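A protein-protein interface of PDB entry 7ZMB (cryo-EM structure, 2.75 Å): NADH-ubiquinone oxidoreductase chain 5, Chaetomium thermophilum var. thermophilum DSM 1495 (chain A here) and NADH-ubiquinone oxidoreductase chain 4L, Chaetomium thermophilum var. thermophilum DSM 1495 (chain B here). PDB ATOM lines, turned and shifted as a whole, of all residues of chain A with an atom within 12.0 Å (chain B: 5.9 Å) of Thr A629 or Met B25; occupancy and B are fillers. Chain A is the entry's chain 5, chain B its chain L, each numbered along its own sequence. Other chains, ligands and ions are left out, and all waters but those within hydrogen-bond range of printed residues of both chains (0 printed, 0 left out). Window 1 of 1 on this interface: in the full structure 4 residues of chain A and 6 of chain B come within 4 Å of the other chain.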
ATOM      1  N   LEU A 623      40.042   1.219   6.995  1.00  0.00           N
ATOM      2  CA  LEU A 623      38.770   0.636   7.388  1.00  0.00           C
ATOM      3  C   LEU A 623      38.922  -0.787   7.881  1.00  0.00           C
ATOM      4  O   LEU A 623      37.973  -1.340   8.442  1.00  0.00           O
ATOM      5  CB  LEU A 623      37.802   0.654   6.211  1.00  0.00           C
ATOM      6  CG  LEU A 623      37.118   1.960   5.855  1.00  0.00           C
ATOM      7  CD1 LEU A 623      38.103   2.897   5.259  1.00  0.00           C
ATOM      8  CD2 LEU A 623      36.045   1.671   4.854  1.00  0.00           C
ATOM      9  N   SER A 624      40.081  -1.394   7.675  1.00  0.00           N
ATOM     10  CA  SER A 624      40.277  -2.802   7.990  1.00  0.00           C
ATOM     11  C   SER A 624      40.827  -2.888   9.408  1.00  0.00           C
ATOM     12  O   SER A 624      41.954  -3.317   9.646  1.00  0.00           O
ATOM     13  CB  SER A 624      41.190  -3.450   6.956  1.00  0.00           C
ATOM     14  OG  SER A 624      41.112  -4.859   6.992  1.00  0.00           O
ATOM     15  N   THR A 625      40.003  -2.481  10.363  1.00  0.00           N
ATOM     16  CA  THR A 625      40.356  -2.451  11.775  1.00  0.00           C
ATOM     17  C   THR A 625      40.216  -3.807  12.460  1.00  0.00           C
ATOM     18  O   THR A 625      40.580  -3.933  13.628  1.00  0.00           O
ATOM     19  CB  THR A 625      39.489  -1.412  12.490  1.00  0.00           C
ATOM     20  OG1 THR A 625      39.927  -1.258  13.842  1.00  0.00           O
ATOM     21  CG2 THR A 625      38.040  -1.834  12.462  1.00  0.00           C
ATOM     22  N   SER A 626      39.686  -4.808  11.761  1.00  0.00           N
ATOM     23  CA  SER A 626      39.581  -6.188  12.230  1.00  0.00           C
ATOM     24  C   SER A 626      38.682  -6.336  13.457  1.00  0.00           C
ATOM     25  O   SER A 626      38.883  -7.236  14.275  1.00  0.00           O
ATOM     26  CB  SER A 626      40.964  -6.774  12.514  1.00  0.00           C
ATOM     27  OG  SER A 626      40.849  -8.125  12.881  1.00  0.00           O
ATOM     28  N   HIS A 627      37.684  -5.474  13.606  1.00  0.00           N
ATOM     29  CA  HIS A 627      36.720  -5.562  14.693  1.00  0.00           C
ATOM     30  C   HIS A 627      35.382  -5.987  14.106  1.00  0.00           C
ATOM     31  O   HIS A 627      34.921  -5.405  13.123  1.00  0.00           O
ATOM     32  CB  HIS A 627      36.616  -4.227  15.429  1.00  0.00           C
ATOM     33  CG  HIS A 627      35.952  -4.317  16.764  1.00  0.00           C
ATOM     34  ND1 HIS A 627      34.643  -3.941  16.971  1.00  0.00           N
ATOM     35  CD2 HIS A 627      36.416  -4.748  17.961  1.00  0.00           C
ATOM     36  CE1 HIS A 627      34.333  -4.126  18.242  1.00  0.00           C
ATOM     37  NE2 HIS A 627      35.390  -4.615  18.864  1.00  0.00           N
ATOM     38  N   VAL A 628      34.774  -7.011  14.707  1.00  0.00           N
ATOM     39  CA  VAL A 628      33.699  -7.751  14.051  1.00  0.00           C
ATOM     40  C   VAL A 628      32.431  -6.917  13.927  1.00  0.00           C
ATOM     41  O   VAL A 628      31.703  -7.032  12.932  1.00  0.00           O
ATOM     42  CB  VAL A 628      33.442  -9.077  14.792  1.00  0.00           C
ATOM     43  CG1 VAL A 628      33.039  -8.820  16.242  1.00  0.00           C
ATOM     44  CG2 VAL A 628      32.383  -9.892  14.080  1.00  0.00           C
ATOM     45  N   THR A 629      32.226  -6.013  14.884  1.00  0.00           N
ATOM     46  CA  THR A 629      30.998  -5.187  14.853  1.00  0.00           C
ATOM     47  C   THR A 629      31.098  -4.187  13.690  1.00  0.00           C
ATOM     48  O   THR A 629      30.093  -4.009  12.978  1.00  0.00           O
ATOM     49  CB  THR A 629      30.580  -4.742  16.265  1.00  0.00           C
ATOM     50  OG1 THR A 629      31.610  -4.010  16.928  1.00  0.00           O
ATOM     51  CG2 THR A 629      30.165  -5.908  17.136  1.00  0.00           C
ATOM     52  N   THR A 630      32.289  -3.630  13.457  1.00  0.00           N
ATOM     53  CA  THR A 630      32.480  -2.651  12.353  1.00  0.00           C
ATOM     54  C   THR A 630      32.251  -3.376  11.041  1.00  0.00           C
ATOM     55  O   THR A 630      31.614  -2.807  10.146  1.00  0.00           O
ATOM     56  CB  THR A 630      33.885  -2.039  12.388  1.00  0.00           C
ATOM     57  OG1 THR A 630      34.066  -1.535  13.709  1.00  0.00           O
ATOM     58  CG2 THR A 630      34.087  -0.939  11.371  1.00  0.00           C
ATOM     59  N   TYR A 631      32.759  -4.600  10.963  1.00  0.00           N
ATOM     60  CA  TYR A 631      32.644  -5.393   9.722  1.00  0.00           C
ATOM     61  C   TYR A 631      31.180  -5.719   9.423  1.00  0.00           C
ATOM     62  O   TYR A 631      30.810  -5.701   8.248  1.00  0.00           O
ATOM     63  CB  TYR A 631      33.557  -6.610   9.823  1.00  0.00           C
ATOM     64  CG  TYR A 631      35.005  -6.323   9.530  1.00  0.00           C
ATOM     65  CD1 TYR A 631      35.440  -5.039   9.248  1.00  0.00           C
ATOM     66  CD2 TYR A 631      35.933  -7.346   9.530  1.00  0.00           C
ATOM     67  CE1 TYR A 631      36.773  -4.776   8.979  1.00  0.00           C
ATOM     68  CE2 TYR A 631      37.264  -7.098   9.260  1.00  0.00           C
ATOM     69  CZ  TYR A 631      37.682  -5.812   8.983  1.00  0.00           C
ATOM     70  OH  TYR A 631      39.002  -5.601   8.723  1.00  0.00           O
ATOM     71  N   ALA A 632      30.398  -6.047  10.455  1.00  0.00           N
ATOM     72  CA  ALA A 632      28.964  -6.374  10.270  1.00  0.00           C
ATOM     73  C   ALA A 632      28.245  -5.142   9.743  1.00  0.00           C
ATOM     74  O   ALA A 632      27.393  -5.300   8.862  1.00  0.00           O
ATOM     75  CB  ALA A 632      28.346  -6.866  11.549  1.00  0.00           C
ATOM     76  N   LEU A 633      28.571  -3.976  10.287  1.00  0.00           N
ATOM     77  CA  LEU A 633      27.955  -2.709   9.825  1.00  0.00           C
ATOM     78  C   LEU A 633      28.338  -2.472   8.362  1.00  0.00           C
ATOM     79  O   LEU A 633      27.453  -2.097   7.592  1.00  0.00           O
ATOM     80  CB  LEU A 633      28.408  -1.572  10.741  1.00  0.00           C
ATOM     81  CG  LEU A 633      27.774  -0.209  10.469  1.00  0.00           C
ATOM     82  CD1 LEU A 633      26.277  -0.331  10.234  1.00  0.00           C
ATOM     83  CD2 LEU A 633      28.057   0.746  11.612  1.00  0.00           C
ATOM     84  N   TYR A 634      29.576  -2.763   7.979  1.00  0.00           N
ATOM     85  CA  TYR A 634      29.955  -2.636   6.549  1.00  0.00           C
ATOM     86  C   TYR A 634      29.086  -3.584   5.708  1.00  0.00           C
ATOM     87  O   TYR A 634      28.598  -3.152   4.644  1.00  0.00           O
ATOM     88  CB  TYR A 634      31.427  -3.000   6.354  1.00  0.00           C
ATOM     89  CG  TYR A 634      32.479  -2.108   6.958  1.00  0.00           C
ATOM     90  CD1 TYR A 634      32.189  -0.851   7.457  1.00  0.00           C
ATOM     91  CD2 TYR A 634      33.797  -2.534   7.009  1.00  0.00           C
ATOM     92  CE1 TYR A 634      33.179  -0.052   8.003  1.00  0.00           C
ATOM     93  CE2 TYR A 634      34.796  -1.742   7.545  1.00  0.00           C
ATOM     94  CZ  TYR A 634      34.490  -0.490   8.038  1.00  0.00           C
ATOM     95  OH  TYR A 634      35.478   0.281   8.571  1.00  0.00           O
ATOM     96  N   ILE A 635      28.881  -4.823   6.177  1.00  0.00           N
ATOM     97  CA  ILE A 635      28.072  -5.827   5.417  1.00  0.00           C
ATOM     98  C   ILE A 635      26.631  -5.339   5.295  1.00  0.00           C
ATOM     99  O   ILE A 635      26.071  -5.475   4.199  1.00  0.00           O
ATOM    100  CB  ILE A 635      28.163  -7.239   6.017  1.00  0.00           C
ATOM    101  CG1 ILE A 635      29.569  -7.814   5.867  1.00  0.00           C
ATOM    102  CG2 ILE A 635      27.118  -8.165   5.406  1.00  0.00           C
ATOM    103  CD1 ILE A 635      29.816  -9.015   6.736  1.00  0.00           C
ATOM    104  N   LEU A 636      26.072  -4.795   6.381  1.00  0.00           N
ATOM    105  CA  LEU A 636      24.698  -4.306   6.367  1.00  0.00           C
ATOM    106  C   LEU A 636      24.554  -3.082   5.476  1.00  0.00           C
ATOM    107  O   LEU A 636      23.523  -2.903   4.823  1.00  0.00           O
ATOM    108  CB  LEU A 636      24.242  -3.997   7.792  1.00  0.00           C
ATOM    109  CG  LEU A 636      22.857  -3.392   8.021  1.00  0.00           C
ATOM    110  CD1 LEU A 636      21.786  -4.276   7.439  1.00  0.00           C
ATOM    111  CD2 LEU A 636      22.632  -3.196   9.489  1.00  0.00           C
ATOM    112  N   VAL A 637      25.573  -2.227   5.435  1.00  0.00           N
ATOM    113  CA  VAL A 637      25.532  -1.067   4.552  1.00  0.00           C
ATOM    114  C   VAL A 637      25.516  -1.501   3.092  1.00  0.00           C
ATOM    115  O   VAL A 637      24.738  -0.979   2.284  1.00  0.00           O
ATOM    116  CB  VAL A 637      26.710  -0.127   4.855  1.00  0.00           C
ATOM    117  CG1 VAL A 637      26.867   0.907   3.762  1.00  0.00           C
ATOM    118  CG2 VAL A 637      26.489   0.538   6.180  1.00  0.00           C
ATOM    119  N   GLY A 638      26.369  -2.458   2.729  1.00  0.00           N
ATOM    120  CA  GLY A 638      26.354  -2.963   1.369  1.00  0.00           C
ATOM    121  C   GLY A 638      25.066  -3.692   1.046  1.00  0.00           C
ATOM    122  O   GLY A 638      24.568  -3.627  -0.081  1.00  0.00           O
ATOM    123  N   GLY B  14      20.695  -5.923  16.791  1.00  0.00           N
ATOM    124  CA  GLY B  14      21.321  -6.495  17.961  1.00  0.00           C
ATOM    125  C   GLY B  14      22.582  -7.267  17.653  1.00  0.00           C
ATOM    126  O   GLY B  14      23.313  -7.624  18.582  1.00  0.00           O
ATOM    127  N   PHE B  15      22.829  -7.562  16.379  1.00  0.00           N
ATOM    128  CA  PHE B  15      24.076  -8.137  15.900  1.00  0.00           C
ATOM    129  C   PHE B  15      25.044  -7.056  15.443  1.00  0.00           C
ATOM    130  O   PHE B  15      26.231  -7.108  15.766  1.00  0.00           O
ATOM    131  CB  PHE B  15      23.783  -9.112  14.754  1.00  0.00           C
ATOM    132  CG  PHE B  15      24.991  -9.801  14.210  1.00  0.00           C
ATOM    133  CD1 PHE B  15      25.489 -10.944  14.823  1.00  0.00           C
ATOM    134  CD2 PHE B  15      25.634  -9.314  13.083  1.00  0.00           C
ATOM    135  CE1 PHE B  15      26.602 -11.590  14.326  1.00  0.00           C
ATOM    136  CE2 PHE B  15      26.751  -9.948  12.583  1.00  0.00           C
ATOM    137  CZ  PHE B  15      27.235 -11.092  13.205  1.00  0.00           C
ATOM    138  N   VAL B  16      24.550  -6.058  14.721  1.00  0.00           N
ATOM    139  CA  VAL B  16      25.429  -5.051  14.145  1.00  0.00           C
ATOM    140  C   VAL B  16      25.640  -3.857  15.066  1.00  0.00           C
ATOM    141  O   VAL B  16      26.721  -3.260  15.060  1.00  0.00           O
ATOM    142  CB  VAL B  16      24.891  -4.606  12.780  1.00  0.00           C
ATOM    143  CG1 VAL B  16      25.895  -3.790  12.100  1.00  0.00           C
ATOM    144  CG2 VAL B  16      24.610  -5.813  11.922  1.00  0.00           C
ATOM    145  N   ASN B  18      25.582  -4.021  18.310  1.00  0.00           N
ATOM    146  CA  ASN B  18      25.850  -4.529  19.684  1.00  0.00           C
ATOM    147  C   ASN B  18      27.269  -4.166  20.106  1.00  0.00           C
ATOM    148  O   ASN B  18      28.180  -4.415  19.319  1.00  0.00           O
ATOM    149  CB  ASN B  18      25.698  -6.057  19.722  1.00  0.00           C
ATOM    150  CG  ASN B  18      26.191  -6.712  20.996  1.00  0.00           C
ATOM    151  OD1 ASN B  18      26.264  -6.079  22.043  1.00  0.00           O
ATOM    152  ND2 ASN B  18      26.524  -7.986  20.916  1.00  0.00           N
ATOM    153  N   ARG B  19      27.423  -3.550  21.278  1.00  0.00           N
ATOM    154  CA  ARG B  19      28.755  -3.100  21.766  1.00  0.00           C
ATOM    155  C   ARG B  19      28.981  -3.689  23.170  1.00  0.00           C
ATOM    156  O   ARG B  19      29.615  -3.011  24.003  1.00  0.00           O
ATOM    157  CB  ARG B  19      28.905  -1.582  21.602  1.00  0.00           C
ATOM    158  CG  ARG B  19      29.204  -1.113  20.186  1.00  0.00           C
ATOM    159  CD  ARG B  19      27.984  -0.889  19.300  1.00  0.00           C
ATOM    160  NE  ARG B  19      28.283  -0.501  17.926  1.00  0.00           N
ATOM    161  CZ  ARG B  19      28.148   0.729  17.439  1.00  0.00           C
ATOM    162  NH1 ARG B  19      28.455   0.982  16.176  1.00  0.00           N
ATOM    163  NH2 ARG B  19      27.698   1.699  18.216  1.00  0.00           N
ATOM    164  N   ASN B  21      29.108  -7.794  24.045  1.00  0.00           N
ATOM    165  CA  ASN B  21      29.834  -9.055  24.133  1.00  0.00           C
ATOM    166  C   ASN B  21      29.360  -9.991  23.030  1.00  0.00           C
ATOM    167  O   ASN B  21      28.318  -9.776  22.408  1.00  0.00           O
ATOM    168  CB  ASN B  21      29.680  -9.711  25.514  1.00  0.00           C
ATOM    169  CG  ASN B  21      28.242 -10.004  25.876  1.00  0.00           C
ATOM    170  OD1 ASN B  21      27.496 -10.596  25.105  1.00  0.00           O
ATOM    171  ND2 ASN B  21      27.837  -9.564  27.056  1.00  0.00           N
ATOM    172  N   ILE B  22      30.142 -11.048  22.808  1.00  0.00           N
ATOM    173  CA  ILE B  22      29.915 -11.929  21.670  1.00  0.00           C
ATOM    174  C   ILE B  22      28.802 -12.944  21.918  1.00  0.00           C
ATOM    175  O   ILE B  22      28.234 -13.471  20.954  1.00  0.00           O
ATOM    176  CB  ILE B  22      31.237 -12.621  21.291  1.00  0.00           C
ATOM    177  CG1 ILE B  22      32.327 -11.576  21.062  1.00  0.00           C
ATOM    178  CG2 ILE B  22      31.091 -13.488  20.049  1.00  0.00           C
ATOM    179  CD1 ILE B  22      33.714 -12.055  21.395  1.00  0.00           C
ATOM    180  N   ILE B  23      28.458 -13.244  23.172  1.00  0.00           N
ATOM    181  CA  ILE B  23      27.286 -14.089  23.383  1.00  0.00           C
ATOM    182  C   ILE B  23      26.030 -13.360  22.922  1.00  0.00           C
ATOM    183  O   ILE B  23      25.109 -13.978  22.383  1.00  0.00           O
ATOM    184  CB  ILE B  23      27.186 -14.556  24.851  1.00  0.00           C
ATOM    185  CG1 ILE B  23      28.368 -15.452  25.193  1.00  0.00           C
ATOM    186  CG2 ILE B  23      25.908 -15.345  25.083  1.00  0.00           C
ATOM    187  CD1 ILE B  23      28.239 -16.213  26.486  1.00  0.00           C
ATOM    188  N   LEU B  24      25.978 -12.040  23.103  1.00  0.00           N
ATOM    189  CA  LEU B  24      24.855 -11.275  22.572  1.00  0.00           C
ATOM    190  C   LEU B  24      24.904 -11.174  21.055  1.00  0.00           C
ATOM    191  O   LEU B  24      23.855 -11.072  20.413  1.00  0.00           O
ATOM    192  CB  LEU B  24      24.813  -9.882  23.184  1.00  0.00           C
ATOM    193  CG  LEU B  24      23.399  -9.309  23.202  1.00  0.00           C
ATOM    194  CD1 LEU B  24      22.442 -10.287  23.869  1.00  0.00           C
ATOM    195  CD2 LEU B  24      23.365  -7.954  23.886  1.00  0.00           C
ATOM    196  N   MET B  25      26.102 -11.177  20.473  1.00  0.00           N
ATOM    197  CA  MET B  25      26.233 -11.364  19.032  1.00  0.00           C
ATOM    198  C   MET B  25      25.563 -12.659  18.603  1.00  0.00           C
ATOM    199  O   MET B  25      24.707 -12.675  17.714  1.00  0.00           O
ATOM    200  CB  MET B  25      27.714 -11.395  18.660  1.00  0.00           C
ATOM    201  CG  MET B  25      28.473 -10.112  18.875  1.00  0.00           C
ATOM    202  SD  MET B  25      27.865  -8.749  17.906  1.00  0.00           S
ATOM    203  CE  MET B  25      28.374  -9.307  16.284  1.00  0.00           C
ATOM    204  N   LEU B  26      25.935 -13.753  19.260  1.00  0.00           N
ATOM    205  CA  LEU B  26      25.446 -15.082  18.929  1.00  0.00           C
ATOM    206  C   LEU B  26      23.966 -15.247  19.264  1.00  0.00           C
ATOM    207  O   LEU B  26      23.277 -16.051  18.631  1.00  0.00           O
ATOM    208  CB  LEU B  26      26.324 -16.095  19.661  1.00  0.00           C
ATOM    209  CG  LEU B  26      26.017 -17.563  19.890  1.00  0.00           C
ATOM    210  CD1 LEU B  26      26.111 -18.362  18.611  1.00  0.00           C
ATOM    211  CD2 LEU B  26      27.004 -18.072  20.910  1.00  0.00           C
ATOM    212  N   ILE B  27      23.463 -14.490  20.243  1.00  0.00           N
ATOM    213  CA  ILE B  27      22.032 -14.469  20.535  1.00  0.00           C
ATOM    214  C   ILE B  27      21.255 -13.832  19.390  1.00  0.00           C
ATOM    215  O   ILE B  27      20.180 -14.305  19.010  1.00  0.00           O
ATOM    216  CB  ILE B  27      21.770 -13.731  21.859  1.00  0.00           C
ATOM    217  CG1 ILE B  27      22.023 -14.639  23.054  1.00  0.00           C
ATOM    218  CG2 ILE B  27      20.361 -13.191  21.905  1.00  0.00           C
ATOM    219  CD1 ILE B  27      21.716 -13.992  24.360  1.00  0.00           C
ATOM    220  N   SER B  28      21.770 -12.738  18.837  1.00  0.00           N
ATOM    221  CA  SER B  28      21.011 -12.005  17.831  1.00  0.00           C
ATOM    222  C   SER B  28      20.855 -12.799  16.544  1.00  0.00           C
ATOM    223  O   SER B  28      19.862 -12.623  15.831  1.00  0.00           O
ATOM    224  CB  SER B  28      21.675 -10.665  17.557  1.00  0.00           C
ATOM    225  OG  SER B  28      21.635  -9.874  18.722  1.00  0.00           O
ATOM    226  N   ILE B  29      21.816 -13.663  16.223  1.00  0.00           N
ATOM    227  CA  ILE B  29      21.617 -14.593  15.118  1.00  0.00           C
ATOM    228  C   ILE B  29      20.435 -15.502  15.414  1.00  0.00           C
ATOM    229  O   ILE B  29      19.585 -15.744  14.551  1.00  0.00           O
ATOM    230  CB  ILE B  29      22.902 -15.396  14.859  1.00  0.00           C
ATOM    231  CG1 ILE B  29      23.895 -14.563  14.047  1.00  0.00           C
ATOM    232  CG2 ILE B  29      22.587 -16.701  14.158  1.00  0.00           C
ATOM    233  CD1 ILE B  29      25.339 -14.934  14.289  1.00  0.00           C
ATOM    234  N   GLU B  30      20.354 -15.978  16.657  1.00  0.00           N
ATOM    235  CA  GLU B  30      19.258 -16.868  17.092  1.00  0.00           C
ATOM    236  C   GLU B  30      17.911 -16.159  16.939  1.00  0.00           C
ATOM    237  O   GLU B  30      16.927 -16.844  16.666  1.00  0.00           O
ATOM    238  CB  GLU B  30      19.484 -17.245  18.550  1.00  0.00           C
ATOM    239  CG  GLU B  30      20.765 -18.000  18.830  1.00  0.00           C
ATOM    240  CD  GLU B  30      20.913 -18.388  20.292  1.00  0.00           C
ATOM    241  OE1 GLU B  30      19.930 -18.227  21.045  1.00  0.00           O
ATOM    242  OE2 GLU B  30      22.010 -18.840  20.677  1.00  0.00           O
ATOM    243  N   ILE B  86      33.413  -7.062  23.627  1.00  0.00           N
ATOM    244  CA  ILE B  86      33.830  -6.376  22.418  1.00  0.00           C
ATOM    245  C   ILE B  86      34.133  -4.921  22.749  1.00  0.00           C
ATOM    246  O   ILE B  86      33.338  -4.228  23.403  1.00  0.00           O
ATOM    247  CB  ILE B  86      32.749  -6.533  21.337  1.00  0.00           C
ATOM    248  CG1 ILE B  86      31.434  -5.912  21.783  1.00  0.00           C
ATOM    249  CG2 ILE B  86      32.515  -8.004  21.024  1.00  0.00           C
ATOM    250  CD1 ILE B  86      30.448  -5.883  20.685  1.00  0.00           C
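Among the printed residues, merely in contact across the chains: Thr A629 with Asn B18 (3.3 Å), Thr A629 with Met B25 (3.7 Å), Thr A629 with Ile B86 (3.6 Å), Ala A632 with Phe B15 (3.6 Å), Ala A632 with Val B16 (3.6 Å) and Leu A633 with Val B16 (3.2 Å).
Of the 16 printed residues of chain A, 3 touch a printed residue of chain B.
Hydrophobic or aromatic side chains of chain A that line the printed part of chain B: Ala A632 and Leu A633.
Hydrophobic or aromatic side chains of chain B that line the printed part of chain A: Phe B15, Val B16, Met B25 and Ile B86.
The side-chain amide nitrogen of Asn B18 sits at hydrogen-bond distance from the backbone carbonyl oxygen of Asn B21 (2.9 Å).
N of Met B25 sits close to ND2 of Asn B18, at 3.2 Å.
The side-chain hydroxyl (OG1) of Thr A629 lies close to a ring nitrogen (ND1) of His A627 (3.0 Å).
Of chain A, only Thr A629 comes within 4 Å of Met B25.
No residue of chain A comes within 4 Å of Gly B14.
Phe B15 touches just one residue of chain A: Ala A632.
Of chain A, only Thr A629 comes within 4 Å of Asn B18.
No residue of chain A comes within 4 Å of Arg B19.
No residue of chain A comes within 4 Å of Asn B21.
No residue of chain A comes within 4 Å of Leu B26.
No residue of chain A comes within 4 Å of Ile B27.
No residue of chain A comes within 4 Å of Ser B28.
No residue of chain A comes within 4 Å of Ile B29.
Printed residues of chain B within 4 Å of Leu A633: Val B16.
Printed residues of chain B within 4 Å of Ala A632: Phe B15 (3.6 Å) and Val B16 (3.6 Å).
Val A628 touches none of the printed residues of chain B.
Thr A625 touches none of the printed residues of chain B.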
